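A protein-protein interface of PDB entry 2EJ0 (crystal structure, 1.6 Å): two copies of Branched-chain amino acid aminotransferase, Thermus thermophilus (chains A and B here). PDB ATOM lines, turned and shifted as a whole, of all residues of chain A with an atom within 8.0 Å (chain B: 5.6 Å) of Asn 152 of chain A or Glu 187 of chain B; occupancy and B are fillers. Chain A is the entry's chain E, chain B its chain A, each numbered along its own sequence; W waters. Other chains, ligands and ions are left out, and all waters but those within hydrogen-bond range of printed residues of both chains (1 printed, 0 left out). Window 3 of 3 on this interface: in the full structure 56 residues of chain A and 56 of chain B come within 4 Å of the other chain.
Of the 11 printed residues of chain A, 4 touch a printed residue of chain B.
Hydrophobic or aromatic side chains of chain A that line the printed part of chain B: Pro 150 and Val 153.
Among the printed residues, 9 pairs touch across the chains.
Among the printed residues, no Asp or Glu carboxylate lies within 4 Å of a Lys or Arg side-chain nitrogen of the other chain.
Printed residues of chain B within 4 Å of Asn 152 of chain A: Trp 146, Ala 147 and Glu 187.
Of chain A, only Pro 150 (3.0 Å), Asn 152 (2.6 Å) and Val 153 (3.5 Å) come within 4 Å of Glu 187 of chain B.
Printed residues of chain B within 4 Å of Val 153 of chain A: Trp 146 (3.8 Å), Ala 147 (3.6 Å), Asn 166 (2.8 Å) and Glu 187 (3.5 Å).
Of the printed residues of chain A, Asn 166 of chain B touches Val 153 (2.8 Å).
Of the printed residues of chain B, Pro 150 of chain A touches Glu 187 (3.0 Å).
Of the printed residues of chain A, Pro 150 of chain B touches Glu 187.
Gly 189 of chain B touches none of the printed residues of chain A.
Gly 156 of chain A touches none of the printed residues of chain B.
The nearest printed residue of chain A that does not touch Trp 146 of chain B is Ala 151 of chain A (4.1 Å).
The backbone carbonyl oxygen (O) of Ala 147 of chain B is in hydrogen-bond range of the side-chain amide nitrogen (ND2) of Asn 166 of chain B, at 2.9 Å.
The guanidinium group (NH1) of Arg 148 of chain B lies within hydrogen-bond range of the side-chain amide oxygen (OD1) of Asn 166 of chain B (2.8 Å).
The backbone NH of Ala 147 of chain B lies within hydrogen-bond range of the backbone carbonyl oxygen of Asn 152 of chain A (2.8 Å).
O of Val 153 of chain A sits at hydrogen-bond distance from ND2 of Asn 166 of chain B (2.8 Å).
The side-chain carboxylate of Glu 187 of chain B sits close to the side-chain amide oxygen of Asn 152 of chain A.
Among the printed residues, merely in contact across the chains: Pro 150 of chain A with Glu 187 of chain B (3.0 Å), Asn 152 of chain A with Trp 146 of chain B (3.4 Å), Val 153 of chain A with Trp 146 of chain B (3.8 Å), Val 153 of chain A with Ala 147 of chain B (3.6 Å), Val 153 of chain A with Glu 187 of chain B (3.5 Å) and Glu 187 of chain A with Pro 150 of chain B (3.0 Å).
Pro 150 of chain A touches Glu 187 of chain B, and with the chains exchanged Glu 187 of chain A touches Pro 150 of chain B.
3 positions are printed for both chains.
Water W1 bridges O of Ser 145 of chain B (2.6 Å) and ND2 of Asn 152 of chain A (2.9 Å).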
ATOM      1  N   PHE A 149      -9.466  -2.384  20.489  1.00  0.00           N
ATOM      2  CA  PHE A 149      -9.339  -2.623  21.918  1.00  0.00           C
ATOM      3  C   PHE A 149      -9.821  -3.966  22.459  1.00  0.00           C
ATOM      4  O   PHE A 149     -10.851  -4.492  22.037  1.00  0.00           O
ATOM      5  CB  PHE A 149     -10.047  -1.495  22.678  1.00  0.00           C
ATOM      6  CG  PHE A 149     -11.233  -0.925  21.951  1.00  0.00           C
ATOM      7  CD1 PHE A 149     -12.351  -1.711  21.691  1.00  0.00           C
ATOM      8  CD2 PHE A 149     -11.221   0.392  21.497  1.00  0.00           C
ATOM      9  CE1 PHE A 149     -13.438  -1.196  20.992  1.00  0.00           C
ATOM     10  CE2 PHE A 149     -12.302   0.915  20.797  1.00  0.00           C
ATOM     11  CZ  PHE A 149     -13.412   0.121  20.544  1.00  0.00           C
ATOM     12  N   PRO A 150      -9.046  -4.556  23.386  1.00  0.00           N
ATOM     13  CA  PRO A 150      -9.422  -5.833  23.997  1.00  0.00           C
ATOM     14  C   PRO A 150     -10.742  -5.602  24.731  1.00  0.00           C
ATOM     15  O   PRO A 150     -11.060  -4.464  25.096  1.00  0.00           O
ATOM     16  CB  PRO A 150      -8.278  -6.096  24.964  1.00  0.00           C
ATOM     17  CG  PRO A 150      -7.099  -5.571  24.219  1.00  0.00           C
ATOM     18  CD  PRO A 150      -7.624  -4.254  23.646  1.00  0.00           C
ATOM     19  N   ALA A 151     -11.491  -6.677  24.962  1.00  0.00           N
ATOM     20  CA  ALA A 151     -12.793  -6.594  25.620  1.00  0.00           C
ATOM     21  C   ALA A 151     -12.771  -6.151  27.079  1.00  0.00           C
ATOM     22  O   ALA A 151     -13.830  -5.936  27.675  1.00  0.00           O
ATOM     23  CB  ALA A 151     -13.519  -7.931  25.493  1.00  0.00           C
ATOM     24  N   ASN A 152     -11.582  -6.031  27.661  1.00  0.00           N
ATOM     25  CA  ASN A 152     -11.465  -5.583  29.046  1.00  0.00           C
ATOM     26  C   ASN A 152     -10.701  -4.264  29.108  1.00  0.00           C
ATOM     27  O   ASN A 152     -10.172  -3.889  30.153  1.00  0.00           O
ATOM     28  CB  ASN A 152     -10.763  -6.646  29.905  1.00  0.00           C
ATOM     29  CG  ASN A 152      -9.330  -6.892  29.475  1.00  0.00           C
ATOM     30  OD1 ASN A 152      -8.950  -6.592  28.345  1.00  0.00           O
ATOM     31  ND2 ASN A 152      -8.531  -7.453  30.375  1.00  0.00           N
ATOM     32  N   VAL A 153     -10.651  -3.561  27.978  1.00  0.00           N
ATOM     33  CA  VAL A 153      -9.966  -2.274  27.894  1.00  0.00           C
ATOM     34  C   VAL A 153     -10.989  -1.182  27.564  1.00  0.00           C
ATOM     35  O   VAL A 153     -11.042  -0.151  28.229  1.00  0.00           O
ATOM     36  CB  VAL A 153      -8.853  -2.316  26.829  1.00  0.00           C
ATOM     37  CG1 VAL A 153      -8.291  -0.919  26.593  1.00  0.00           C
ATOM     38  CG2 VAL A 153      -7.739  -3.245  27.305  1.00  0.00           C
ATOM     39  N   MET A 154     -11.794  -1.420  26.533  1.00  0.00           N
ATOM     40  CA  MET A 154     -12.864  -0.498  26.142  1.00  0.00           C
ATOM     41  C   MET A 154     -14.047  -1.402  25.792  1.00  0.00           C
ATOM     42  O   MET A 154     -13.855  -2.509  25.279  1.00  0.00           O
ATOM     43  CB  MET A 154     -12.463   0.349  24.926  1.00  0.00           C
ATOM     44  CG  MET A 154     -11.265   1.285  25.143  1.00  0.00           C
ATOM     45  SD  MET A 154     -11.541   2.699  26.254  1.00  0.00           S
ATOM     46  CE  MET A 154     -12.332   3.870  25.118  1.00  0.00           C
ATOM     47  N   PRO A 155     -15.284  -0.958  26.077  1.00  0.00           N
ATOM     48  CA  PRO A 155     -16.481  -1.759  25.784  1.00  0.00           C
ATOM     49  C   PRO A 155     -16.847  -1.763  24.302  1.00  0.00           C
ATOM     50  O   PRO A 155     -17.635  -0.937  23.845  1.00  0.00           O
ATOM     51  CB  PRO A 155     -17.548  -1.101  26.654  1.00  0.00           C
ATOM     52  CG  PRO A 155     -17.157   0.337  26.612  1.00  0.00           C
ATOM     53  CD  PRO A 155     -15.644   0.301  26.758  1.00  0.00           C
ATOM     54  N   GLY A 156     -16.276  -2.712  23.567  1.00  0.00           N
ATOM     55  CA  GLY A 156     -16.504  -2.803  22.132  1.00  0.00           C
ATOM     56  C   GLY A 156     -17.892  -3.175  21.642  1.00  0.00           C
ATOM     57  O   GLY A 156     -18.157  -3.107  20.439  1.00  0.00           O
ATOM     58  N   GLU A 187      -5.619  -7.403  19.317  1.00  0.00           N
ATOM     59  CA  GLU A 187      -4.264  -7.454  19.859  1.00  0.00           C
ATOM     60  C   GLU A 187      -3.550  -8.778  19.585  1.00  0.00           C
ATOM     61  O   GLU A 187      -2.319  -8.828  19.538  1.00  0.00           O
ATOM     62  CB  GLU A 187      -4.297  -7.169  21.365  1.00  0.00           C
ATOM     63  CG  GLU A 187      -2.968  -6.713  21.967  1.00  0.00           C
ATOM     64  CD  GLU A 187      -2.433  -5.442  21.326  1.00  0.00           C
ATOM     65  OE1 GLU A 187      -1.789  -5.538  20.265  1.00  0.00           O
ATOM     66  OE2 GLU A 187      -2.658  -4.339  21.880  1.00  0.00           O
ATOM     67  N   GLU A 188      -4.323  -9.840  19.388  1.00  0.00           N
ATOM     68  CA  GLU A 188      -3.756 -11.155  19.123  1.00  0.00           C
ATOM     69  C   GLU A 188      -3.356 -11.328  17.661  1.00  0.00           C
ATOM     70  O   GLU A 188      -2.673 -12.289  17.308  1.00  0.00           O
ATOM     71  CB  GLU A 188      -4.745 -12.252  19.532  1.00  0.00           C
ATOM     72  CG  GLU A 188      -4.947 -12.394  21.042  1.00  0.00           C
ATOM     73  CD  GLU A 188      -5.567 -11.162  21.684  1.00  0.00           C
ATOM     74  OE1 GLU A 188      -6.589 -10.667  21.169  1.00  0.00           O
ATOM     75  OE2 GLU A 188      -5.040 -10.696  22.716  1.00  0.00           O
ATOM     76  N   VAL A 214     -14.125  -8.718  19.546  1.00  0.00           N
ATOM     77  CA  VAL A 214     -14.113  -7.413  20.217  1.00  0.00           C
ATOM     78  C   VAL A 214     -14.877  -6.341  19.443  1.00  0.00           C
ATOM     79  O   VAL A 214     -14.815  -5.157  19.783  1.00  0.00           O
ATOM     80  CB  VAL A 214     -12.666  -6.900  20.418  1.00  0.00           C
ATOM     81  CG1 VAL A 214     -11.942  -7.756  21.451  1.00  0.00           C
ATOM     82  CG2 VAL A 214     -11.917  -6.923  19.086  1.00  0.00           C
ATOM     83  N   SER B 145     -10.657  -4.525  37.128  1.00  0.00           N
ATOM     84  CA  SER B 145     -10.910  -5.623  36.206  1.00  0.00           C
ATOM     85  C   SER B 145     -10.805  -5.066  34.789  1.00  0.00           C
ATOM     86  O   SER B 145     -11.009  -5.783  33.808  1.00  0.00           O
ATOM     87  CB  SER B 145     -12.300  -6.219  36.432  1.00  0.00           C
ATOM     88  OG  SER B 145     -13.300  -5.260  36.169  1.00  0.00           O
ATOM     89  N   TRP B 146     -10.512  -3.771  34.696  1.00  0.00           N
ATOM     90  CA  TRP B 146     -10.313  -3.111  33.412  1.00  0.00           C
ATOM     91  C   TRP B 146      -8.810  -2.911  33.270  1.00  0.00           C
ATOM     92  O   TRP B 146      -8.167  -2.338  34.151  1.00  0.00           O
ATOM     93  CB  TRP B 146     -11.029  -1.754  33.363  1.00  0.00           C
ATOM     94  CG  TRP B 146     -12.521  -1.885  33.317  1.00  0.00           C
ATOM     95  CD1 TRP B 146     -13.375  -1.899  34.382  1.00  0.00           C
ATOM     96  CD2 TRP B 146     -13.324  -2.123  32.153  1.00  0.00           C
ATOM     97  NE1 TRP B 146     -14.661  -2.138  33.954  1.00  0.00           N
ATOM     98  CE2 TRP B 146     -14.658  -2.280  32.591  1.00  0.00           C
ATOM     99  CE3 TRP B 146     -13.044  -2.223  30.782  1.00  0.00           C
ATOM    100  CZ2 TRP B 146     -15.714  -2.533  31.706  1.00  0.00           C
ATOM    101  CZ3 TRP B 146     -14.094  -2.476  29.902  1.00  0.00           C
ATOM    102  CH2 TRP B 146     -15.413  -2.628  30.370  1.00  0.00           C
ATOM    103  N   ALA B 147      -8.249  -3.403  32.168  1.00  0.00           N
ATOM    104  CA  ALA B 147      -6.820  -3.272  31.926  1.00  0.00           C
ATOM    105  C   ALA B 147      -6.512  -1.953  31.237  1.00  0.00           C
ATOM    106  O   ALA B 147      -7.307  -1.456  30.435  1.00  0.00           O
ATOM    107  CB  ALA B 147      -6.329  -4.431  31.065  1.00  0.00           C
ATOM    108  N   ARG B 148      -5.358  -1.383  31.564  1.00  0.00           N
ATOM    109  CA  ARG B 148      -4.935  -0.137  30.951  1.00  0.00           C
ATOM    110  C   ARG B 148      -4.673  -0.476  29.488  1.00  0.00           C
ATOM    111  O   ARG B 148      -4.094  -1.518  29.187  1.00  0.00           O
ATOM    112  CB  ARG B 148      -3.657   0.367  31.611  1.00  0.00           C
ATOM    113  CG  ARG B 148      -3.435   1.835  31.432  1.00  0.00           C
ATOM    114  CD  ARG B 148      -4.628   2.582  31.989  1.00  0.00           C
ATOM    115  NE  ARG B 148      -4.426   4.019  31.954  1.00  0.00           N
ATOM    116  CZ  ARG B 148      -5.407   4.910  32.022  1.00  0.00           C
ATOM    117  NH1 ARG B 148      -6.671   4.513  32.129  1.00  0.00           N
ATOM    118  NH2 ARG B 148      -5.117   6.201  31.984  1.00  0.00           N
ATOM    119  N   PRO B 150      -3.327  -1.050  25.759  1.00  0.00           N
ATOM    120  CA  PRO B 150      -2.005  -1.323  25.186  1.00  0.00           C
ATOM    121  C   PRO B 150      -1.586  -0.071  24.412  1.00  0.00           C
ATOM    122  O   PRO B 150      -2.442   0.726  24.011  1.00  0.00           O
ATOM    123  CB  PRO B 150      -2.275  -2.505  24.266  1.00  0.00           C
ATOM    124  CG  PRO B 150      -3.304  -3.273  25.033  1.00  0.00           C
ATOM    125  CD  PRO B 150      -4.247  -2.173  25.503  1.00  0.00           C
ATOM    126  N   ASN B 166     -11.649   4.482  29.892  1.00  0.00           N
ATOM    127  CA  ASN B 166     -10.964   3.388  30.575  1.00  0.00           C
ATOM    128  C   ASN B 166     -10.766   3.777  32.043  1.00  0.00           C
ATOM    129  O   ASN B 166     -11.019   2.978  32.952  1.00  0.00           O
ATOM    130  CB  ASN B 166      -9.619   3.116  29.876  1.00  0.00           C
ATOM    131  CG  ASN B 166      -8.839   1.970  30.506  1.00  0.00           C
ATOM    132  OD1 ASN B 166      -7.866   2.193  31.219  1.00  0.00           O
ATOM    133  ND2 ASN B 166      -9.264   0.737  30.237  1.00  0.00           N
ATOM    134  N   LEU B 185      -3.958  -2.773  35.845  1.00  0.00           N
ATOM    135  CA  LEU B 185      -2.851  -3.594  35.365  1.00  0.00           C
ATOM    136  C   LEU B 185      -2.856  -3.457  33.850  1.00  0.00           C
ATOM    137  O   LEU B 185      -3.863  -3.044  33.274  1.00  0.00           O
ATOM    138  CB  LEU B 185      -3.087  -5.070  35.691  1.00  0.00           C
ATOM    139  CG  LEU B 185      -3.345  -5.477  37.137  1.00  0.00           C
ATOM    140  CD1 LEU B 185      -3.498  -6.996  37.205  1.00  0.00           C
ATOM    141  CD2 LEU B 185      -2.195  -5.012  38.013  1.00  0.00           C
ATOM    142  N   ASP B 186      -1.743  -3.780  33.194  1.00  0.00           N
ATOM    143  CA  ASP B 186      -1.756  -3.737  31.739  1.00  0.00           C
ATOM    144  C   ASP B 186      -2.313  -5.095  31.293  1.00  0.00           C
ATOM    145  O   ASP B 186      -2.589  -5.959  32.131  1.00  0.00           O
ATOM    146  CB  ASP B 186      -0.358  -3.459  31.142  1.00  0.00           C
ATOM    147  CG  ASP B 186       0.713  -4.436  31.605  1.00  0.00           C
ATOM    148  OD1 ASP B 186       0.399  -5.602  31.906  1.00  0.00           O
ATOM    149  OD2 ASP B 186       1.894  -4.021  31.636  1.00  0.00           O
ATOM    150  N   GLU B 187      -2.504  -5.286  29.993  1.00  0.00           N
ATOM    151  CA  GLU B 187      -3.071  -6.537  29.493  1.00  0.00           C
ATOM    152  C   GLU B 187      -2.232  -7.778  29.820  1.00  0.00           C
ATOM    153  O   GLU B 187      -2.762  -8.885  29.887  1.00  0.00           O
ATOM    154  CB  GLU B 187      -3.286  -6.432  27.978  1.00  0.00           C
ATOM    155  CG  GLU B 187      -4.303  -7.417  27.404  1.00  0.00           C
ATOM    156  CD  GLU B 187      -5.685  -7.260  28.016  1.00  0.00           C
ATOM    157  OE1 GLU B 187      -5.918  -7.818  29.106  1.00  0.00           O
ATOM    158  OE2 GLU B 187      -6.538  -6.570  27.414  1.00  0.00           O
ATOM    159  N   GLU B 188      -0.933  -7.586  30.028  1.00  0.00           N
ATOM    160  CA  GLU B 188      -0.034  -8.693  30.341  1.00  0.00           C
ATOM    161  C   GLU B 188      -0.084  -9.068  31.821  1.00  0.00           C
ATOM    162  O   GLU B 188       0.474 -10.086  32.233  1.00  0.00           O
ATOM    163  CB  GLU B 188       1.399  -8.336  29.943  1.00  0.00           C
ATOM    164  CG  GLU B 188       1.633  -8.272  28.433  1.00  0.00           C
ATOM    165  CD  GLU B 188       0.846  -7.161  27.755  1.00  0.00           C
ATOM    166  OE1 GLU B 188       0.895  -6.014  28.242  1.00  0.00           O
ATOM    167  OE2 GLU B 188       0.187  -7.431  26.730  1.00  0.00           O
ATOM    168  N   GLY B 189      -0.741  -8.233  32.619  1.00  0.00           N
ATOM    169  CA  GLY B 189      -0.865  -8.528  34.036  1.00  0.00           C
ATOM    170  C   GLY B 189       0.015  -7.743  34.990  1.00  0.00           C
ATOM    171  O   GLY B 189      -0.063  -7.952  36.199  1.00  0.00           O
HETATM  172  O   HOH W   1      -9.091  -7.490  33.199  1.00  0.00           O
